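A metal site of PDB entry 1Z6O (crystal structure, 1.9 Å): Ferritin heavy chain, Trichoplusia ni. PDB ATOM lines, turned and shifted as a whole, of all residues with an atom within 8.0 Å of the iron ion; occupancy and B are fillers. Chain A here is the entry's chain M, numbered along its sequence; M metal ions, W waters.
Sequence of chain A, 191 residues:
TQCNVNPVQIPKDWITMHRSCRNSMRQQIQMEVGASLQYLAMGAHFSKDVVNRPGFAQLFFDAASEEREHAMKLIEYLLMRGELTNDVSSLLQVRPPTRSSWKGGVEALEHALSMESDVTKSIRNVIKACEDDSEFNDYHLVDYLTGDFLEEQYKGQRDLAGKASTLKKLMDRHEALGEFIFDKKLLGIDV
NE2 of Gln 28 is in hydrogen-bond range of OE1 of Glu 32 (3.0 Å).
Within 4 Å of the iron ion: Glu 32, Glu 67 and His 70.
The nearest printed residue that does not touch the iron ion is Gln 153 (4.05 Å).
Water W1 lies within hydrogen-bond range of the side-chain carboxylate (OE1) of Glu 32 (2.5 Å) and the side-chain amide oxygen (OE1) of Gln 153 (3.4 Å).
OE2 of Glu 32 binds the iron ion.
The iron ion is bound by ND1 of His 70 (2.0 Å).
The iron ion is bound by water W1, 2.1 Å away.
Water W2 binds the iron ion (2.1 Å).
The iron ion is bound by the side-chain carboxylate (OE1) of Glu 67.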
ATOM      1  N   GLN A  28     -15.553  12.453 -25.616  1.00  0.00           N
ATOM      2  CA  GLN A  28     -16.702  11.901 -26.346  1.00  0.00           C
ATOM      3  C   GLN A  28     -18.013  12.489 -25.804  1.00  0.00           C
ATOM      4  O   GLN A  28     -18.947  12.745 -26.555  1.00  0.00           O
ATOM      5  CB  GLN A  28     -16.732  10.368 -26.225  1.00  0.00           C
ATOM      6  CG  GLN A  28     -17.769   9.698 -27.149  1.00  0.00           C
ATOM      7  CD  GLN A  28     -17.464   9.982 -28.607  1.00  0.00           C
ATOM      8  OE1 GLN A  28     -16.322   9.949 -29.014  1.00  0.00           O
ATOM      9  NE2 GLN A  28     -18.499  10.248 -29.408  1.00  0.00           N
ATOM     10  N   MET A  31     -18.545  15.698 -27.343  1.00  0.00           N
ATOM     11  CA  MET A  31     -18.911  15.512 -28.738  1.00  0.00           C
ATOM     12  C   MET A  31     -20.403  15.154 -28.909  1.00  0.00           C
ATOM     13  O   MET A  31     -21.057  15.647 -29.819  1.00  0.00           O
ATOM     14  CB  MET A  31     -18.049  14.434 -29.386  1.00  0.00           C
ATOM     15  CG  MET A  31     -18.321  14.274 -30.876  1.00  0.00           C
ATOM     16  SD  MET A  31     -17.249  13.034 -31.633  1.00  0.00           S
ATOM     17  CE  MET A  31     -17.209  13.642 -33.386  1.00  0.00           C
ATOM     18  N   GLU A  32     -20.920  14.299 -28.025  1.00  0.00           N
ATOM     19  CA  GLU A  32     -22.342  13.912 -28.106  1.00  0.00           C
ATOM     20  C   GLU A  32     -23.209  15.144 -27.848  1.00  0.00           C
ATOM     21  O   GLU A  32     -24.219  15.359 -28.523  1.00  0.00           O
ATOM     22  CB  GLU A  32     -22.690  12.838 -27.067  1.00  0.00           C
ATOM     23  CG  GLU A  32     -21.877  11.545 -27.182  1.00  0.00           C
ATOM     24  CD  GLU A  32     -22.197  10.701 -28.415  1.00  0.00           C
ATOM     25  OE1 GLU A  32     -21.367   9.831 -28.759  1.00  0.00           O
ATOM     26  OE2 GLU A  32     -23.280  10.876 -29.022  1.00  0.00           O
ATOM     27  N   VAL A  33     -22.830  15.961 -26.864  1.00  0.00           N
ATOM     28  CA  VAL A  33     -23.588  17.170 -26.567  1.00  0.00           C
ATOM     29  C   VAL A  33     -23.545  18.115 -27.766  1.00  0.00           C
ATOM     30  O   VAL A  33     -24.575  18.697 -28.142  1.00  0.00           O
ATOM     31  CB  VAL A  33     -23.052  17.860 -25.282  1.00  0.00           C
ATOM     32  CG1 VAL A  33     -23.664  19.267 -25.124  1.00  0.00           C
ATOM     33  CG2 VAL A  33     -23.413  17.007 -24.058  1.00  0.00           C
ATOM     34  N   ALA A  35     -23.261  17.308 -30.836  1.00  0.00           N
ATOM     35  CA  ALA A  35     -24.139  16.748 -31.866  1.00  0.00           C
ATOM     36  C   ALA A  35     -25.599  17.061 -31.512  1.00  0.00           C
ATOM     37  O   ALA A  35     -26.379  17.391 -32.397  1.00  0.00           O
ATOM     38  CB  ALA A  35     -23.929  15.232 -31.999  1.00  0.00           C
ATOM     39  N   SER A  36     -25.982  16.965 -30.229  1.00  0.00           N
ATOM     40  CA  SER A  36     -27.371  17.261 -29.867  1.00  0.00           C
ATOM     41  C   SER A  36     -27.714  18.701 -30.225  1.00  0.00           C
ATOM     42  O   SER A  36     -28.804  18.963 -30.716  1.00  0.00           O
ATOM     43  CB  SER A  36     -27.673  17.020 -28.359  1.00  0.00           C
ATOM     44  OG  SER A  36     -27.171  18.057 -27.508  1.00  0.00           O
ATOM     45  N   TYR A  39     -28.197  19.088 -34.033  1.00  0.00           N
ATOM     46  CA  TYR A  39     -29.492  18.536 -34.458  1.00  0.00           C
ATOM     47  C   TYR A  39     -30.630  19.483 -34.056  1.00  0.00           C
ATOM     48  O   TYR A  39     -31.623  19.588 -34.784  1.00  0.00           O
ATOM     49  CB  TYR A  39     -29.727  17.144 -33.852  1.00  0.00           C
ATOM     50  CG  TYR A  39     -29.031  16.040 -34.626  1.00  0.00           C
ATOM     51  CD1 TYR A  39     -28.246  15.085 -33.975  1.00  0.00           C
ATOM     52  CD2 TYR A  39     -29.226  15.911 -36.004  1.00  0.00           C
ATOM     53  CE1 TYR A  39     -27.665  14.011 -34.683  1.00  0.00           C
ATOM     54  CE2 TYR A  39     -28.645  14.852 -36.721  1.00  0.00           C
ATOM     55  CZ  TYR A  39     -27.882  13.904 -36.055  1.00  0.00           C
ATOM     56  OH  TYR A  39     -27.356  12.852 -36.776  1.00  0.00           O
ATOM     57  N   ALA A  63     -33.490  13.231 -33.088  1.00  0.00           N
ATOM     58  CA  ALA A  63     -32.058  12.933 -33.091  1.00  0.00           C
ATOM     59  C   ALA A  63     -31.332  13.749 -32.016  1.00  0.00           C
ATOM     60  O   ALA A  63     -30.393  13.259 -31.391  1.00  0.00           O
ATOM     61  CB  ALA A  63     -31.445  13.242 -34.477  1.00  0.00           C
ATOM     62  N   GLU A  66     -31.886  12.073 -28.747  1.00  0.00           N
ATOM     63  CA  GLU A  66     -31.140  10.825 -28.696  1.00  0.00           C
ATOM     64  C   GLU A  66     -29.655  11.099 -28.391  1.00  0.00           C
ATOM     65  O   GLU A  66     -29.025  10.358 -27.629  1.00  0.00           O
ATOM     66  CB  GLU A  66     -31.263  10.079 -30.026  1.00  0.00           C
ATOM     67  CG  GLU A  66     -30.732   8.660 -29.999  1.00  0.00           C
ATOM     68  CD  GLU A  66     -31.660   7.703 -29.250  1.00  0.00           C
ATOM     69  OE1 GLU A  66     -31.970   7.957 -28.053  1.00  0.00           O
ATOM     70  OE2 GLU A  66     -32.082   6.689 -29.853  1.00  0.00           O
ATOM     71  N   GLU A  67     -29.075  12.140 -28.989  1.00  0.00           N
ATOM     72  CA  GLU A  67     -27.652  12.436 -28.721  1.00  0.00           C
ATOM     73  C   GLU A  67     -27.484  12.847 -27.257  1.00  0.00           C
ATOM     74  O   GLU A  67     -26.464  12.557 -26.622  1.00  0.00           O
ATOM     75  CB  GLU A  67     -27.128  13.552 -29.629  1.00  0.00           C
ATOM     76  CG  GLU A  67     -27.028  13.160 -31.127  1.00  0.00           C
ATOM     77  CD  GLU A  67     -26.201  11.886 -31.372  1.00  0.00           C
ATOM     78  OE1 GLU A  67     -25.248  11.628 -30.604  1.00  0.00           O
ATOM     79  OE2 GLU A  67     -26.499  11.151 -32.341  1.00  0.00           O
ATOM     80  N   ARG A  68     -28.463  13.559 -26.706  1.00  0.00           N
ATOM     81  CA  ARG A  68     -28.407  13.942 -25.300  1.00  0.00           C
ATOM     82  C   ARG A  68     -28.410  12.662 -24.463  1.00  0.00           C
ATOM     83  O   ARG A  68     -27.694  12.565 -23.458  1.00  0.00           O
ATOM     84  CB  ARG A  68     -29.606  14.830 -24.945  1.00  0.00           C
ATOM     85  CG  ARG A  68     -29.774  15.145 -23.457  1.00  0.00           C
ATOM     86  CD  ARG A  68     -30.857  16.230 -23.261  1.00  0.00           C
ATOM     87  NE  ARG A  68     -31.143  16.500 -21.845  1.00  0.00           N
ATOM     88  CZ  ARG A  68     -32.016  15.831 -21.102  1.00  0.00           C
ATOM     89  NH1 ARG A  68     -32.194  16.155 -19.825  1.00  0.00           N
ATOM     90  NH2 ARG A  68     -32.717  14.829 -21.638  1.00  0.00           N
ATOM     91  N   GLU A  69     -29.226  11.678 -24.851  1.00  0.00           N
ATOM     92  CA  GLU A  69     -29.252  10.404 -24.114  1.00  0.00           C
ATOM     93  C   GLU A  69     -27.889   9.696 -24.227  1.00  0.00           C
ATOM     94  O   GLU A  69     -27.445   9.045 -23.275  1.00  0.00           O
ATOM     95  CB  GLU A  69     -30.332   9.457 -24.659  1.00  0.00           C
ATOM     96  CG  GLU A  69     -31.786   9.912 -24.441  1.00  0.00           C
ATOM     97  CD  GLU A  69     -32.150  10.052 -22.961  1.00  0.00           C
ATOM     98  OE1 GLU A  69     -31.724   9.206 -22.147  1.00  0.00           O
ATOM     99  OE2 GLU A  69     -32.880  11.010 -22.617  1.00  0.00           O
ATOM    100  N   HIS A  70     -27.227   9.790 -25.377  1.00  0.00           N
ATOM    101  CA  HIS A  70     -25.904   9.155 -25.543  1.00  0.00           C
ATOM    102  C   HIS A  70     -24.921   9.776 -24.558  1.00  0.00           C
ATOM    103  O   HIS A  70     -24.117   9.079 -23.939  1.00  0.00           O
ATOM    104  CB  HIS A  70     -25.355   9.344 -26.965  1.00  0.00           C
ATOM    105  CG  HIS A  70     -26.098   8.588 -28.015  1.00  0.00           C
ATOM    106  ND1 HIS A  70     -25.845   8.740 -29.370  1.00  0.00           N
ATOM    107  CD2 HIS A  70     -27.108   7.683 -27.923  1.00  0.00           C
ATOM    108  CE1 HIS A  70     -26.672   7.969 -30.058  1.00  0.00           C
ATOM    109  NE2 HIS A  70     -27.442   7.316 -29.198  1.00  0.00           N
ATOM    110  N   ALA A  71     -24.953  11.108 -24.441  1.00  0.00           N
ATOM    111  CA  ALA A  71     -24.067  11.786 -23.508  1.00  0.00           C
ATOM    112  C   ALA A  71     -24.340  11.286 -22.092  1.00  0.00           C
ATOM    113  O   ALA A  71     -23.416  10.998 -21.327  1.00  0.00           O
ATOM    114  CB  ALA A  71     -24.273  13.300 -23.574  1.00  0.00           C
ATOM    115  N   LEU A  74     -22.835   7.806 -21.348  1.00  0.00           N
ATOM    116  CA  LEU A  74     -21.385   7.811 -21.134  1.00  0.00           C
ATOM    117  C   LEU A  74     -21.073   8.341 -19.738  1.00  0.00           C
ATOM    118  O   LEU A  74     -20.181   7.835 -19.055  1.00  0.00           O
ATOM    119  CB  LEU A  74     -20.692   8.683 -22.196  1.00  0.00           C
ATOM    120  CG  LEU A  74     -20.815   8.120 -23.626  1.00  0.00           C
ATOM    121  CD1 LEU A  74     -20.257   9.147 -24.610  1.00  0.00           C
ATOM    122  CD2 LEU A  74     -20.057   6.789 -23.752  1.00  0.00           C
ATOM    123  N   MET A 115     -21.900  13.868 -39.791  1.00  0.00           N
ATOM    124  CA  MET A 115     -21.754  14.038 -38.347  1.00  0.00           C
ATOM    125  C   MET A 115     -21.689  12.656 -37.683  1.00  0.00           C
ATOM    126  O   MET A 115     -20.880  12.415 -36.798  1.00  0.00           O
ATOM    127  CB  MET A 115     -22.960  14.785 -37.741  1.00  0.00           C
ATOM    128  CG  MET A 115     -23.152  16.236 -38.169  1.00  0.00           C
ATOM    129  SD  MET A 115     -24.798  16.853 -37.637  1.00  0.00           S
ATOM    130  CE  MET A 115     -24.731  16.399 -35.842  1.00  0.00           C
ATOM    131  N   GLU A 116     -22.569  11.750 -38.100  1.00  0.00           N
ATOM    132  CA  GLU A 116     -22.596  10.404 -37.511  1.00  0.00           C
ATOM    133  C   GLU A 116     -21.304   9.665 -37.827  1.00  0.00           C
ATOM    134  O   GLU A 116     -20.749   8.965 -36.987  1.00  0.00           O
ATOM    135  CB  GLU A 116     -23.800   9.597 -38.030  1.00  0.00           C
ATOM    136  CG  GLU A 116     -25.159  10.129 -37.531  1.00  0.00           C
ATOM    137  CD  GLU A 116     -25.223  10.256 -35.996  1.00  0.00           C
ATOM    138  OE1 GLU A 116     -24.611   9.425 -35.294  1.00  0.00           O
ATOM    139  OE2 GLU A 116     -25.897  11.183 -35.494  1.00  0.00           O
ATOM    140  N   VAL A 119     -18.715  10.801 -35.512  1.00  0.00           N
ATOM    141  CA  VAL A 119     -18.916  10.238 -34.168  1.00  0.00           C
ATOM    142  C   VAL A 119     -18.452   8.785 -34.144  1.00  0.00           C
ATOM    143  O   VAL A 119     -17.826   8.348 -33.172  1.00  0.00           O
ATOM    144  CB  VAL A 119     -20.417  10.328 -33.742  1.00  0.00           C
ATOM    145  CG1 VAL A 119     -20.663   9.478 -32.494  1.00  0.00           C
ATOM    146  CG2 VAL A 119     -20.774  11.793 -33.449  1.00  0.00           C
ATOM    147  N   THR A 120     -18.725   8.040 -35.203  1.00  0.00           N
ATOM    148  CA  THR A 120     -18.312   6.636 -35.250  1.00  0.00           C
ATOM    149  C   THR A 120     -16.780   6.532 -35.175  1.00  0.00           C
ATOM    150  O   THR A 120     -16.226   5.712 -34.446  1.00  0.00           O
ATOM    151  CB  THR A 120     -18.794   5.971 -36.557  1.00  0.00           C
ATOM    152  OG1 THR A 120     -20.225   6.057 -36.595  1.00  0.00           O
ATOM    153  CG2 THR A 120     -18.360   4.493 -36.630  1.00  0.00           C
ATOM    154  N   ILE A 123     -15.657   7.330 -31.611  1.00  0.00           N
ATOM    155  CA  ILE A 123     -15.885   6.223 -30.678  1.00  0.00           C
ATOM    156  C   ILE A 123     -14.817   5.142 -30.898  1.00  0.00           C
ATOM    157  O   ILE A 123     -14.315   4.552 -29.942  1.00  0.00           O
ATOM    158  CB  ILE A 123     -17.310   5.619 -30.854  1.00  0.00           C
ATOM    159  CG1 ILE A 123     -18.349   6.633 -30.340  1.00  0.00           C
ATOM    160  CG2 ILE A 123     -17.445   4.297 -30.072  1.00  0.00           C
ATOM    161  CD1 ILE A 123     -19.768   6.350 -30.816  1.00  0.00           C
ATOM    162  N   PHE A 149     -22.700   1.404 -28.359  1.00  0.00           N
ATOM    163  CA  PHE A 149     -22.514   2.609 -29.153  1.00  0.00           C
ATOM    164  C   PHE A 149     -22.249   2.381 -30.632  1.00  0.00           C
ATOM    165  O   PHE A 149     -22.917   2.996 -31.455  1.00  0.00           O
ATOM    166  CB  PHE A 149     -21.423   3.481 -28.532  1.00  0.00           C
ATOM    167  CG  PHE A 149     -21.909   4.267 -27.342  1.00  0.00           C
ATOM    168  CD1 PHE A 149     -22.216   3.631 -26.155  1.00  0.00           C
ATOM    169  CD2 PHE A 149     -22.166   5.637 -27.464  1.00  0.00           C
ATOM    170  CE1 PHE A 149     -22.782   4.342 -25.084  1.00  0.00           C
ATOM    171  CE2 PHE A 149     -22.729   6.349 -26.403  1.00  0.00           C
ATOM    172  CZ  PHE A 149     -23.040   5.705 -25.218  1.00  0.00           C
ATOM    173  N   GLU A 152     -25.420   1.230 -32.521  1.00  0.00           N
ATOM    174  CA  GLU A 152     -26.335   2.321 -32.844  1.00  0.00           C
ATOM    175  C   GLU A 152     -25.774   3.175 -33.999  1.00  0.00           C
ATOM    176  O   GLU A 152     -26.530   3.629 -34.870  1.00  0.00           O
ATOM    177  CB  GLU A 152     -26.538   3.200 -31.611  1.00  0.00           C
ATOM    178  CG  GLU A 152     -27.908   3.851 -31.571  1.00  0.00           C
ATOM    179  CD  GLU A 152     -29.020   2.829 -31.379  1.00  0.00           C
ATOM    180  OE1 GLU A 152     -30.204   3.195 -31.578  1.00  0.00           O
ATOM    181  OE2 GLU A 152     -28.725   1.663 -31.027  1.00  0.00           O
ATOM    182  N   GLN A 153     -24.462   3.389 -34.006  1.00  0.00           N
ATOM    183  CA  GLN A 153     -23.839   4.182 -35.068  1.00  0.00           C
ATOM    184  C   GLN A 153     -23.993   3.563 -36.452  1.00  0.00           C
ATOM    185  O   GLN A 153     -24.381   4.251 -37.393  1.00  0.00           O
ATOM    186  CB  GLN A 153     -22.336   4.390 -34.809  1.00  0.00           C
ATOM    187  CG  GLN A 153     -22.013   5.382 -33.681  1.00  0.00           C
ATOM    188  CD  GLN A 153     -22.778   6.682 -33.835  1.00  0.00           C
ATOM    189  OE1 GLN A 153     -23.686   6.958 -33.051  1.00  0.00           O
ATOM    190  NE2 GLN A 153     -22.429   7.468 -34.851  1.00  0.00           N
HETATM  191 FE    FE M   1     -24.361   9.806 -30.257  1.00  0.00          FE
HETATM  192  O   HOH W   1     -22.968   8.320 -30.020  1.00  0.00           O
HETATM  193  O   HOH W   2     -24.423   9.457 -32.281  1.00  0.00           O
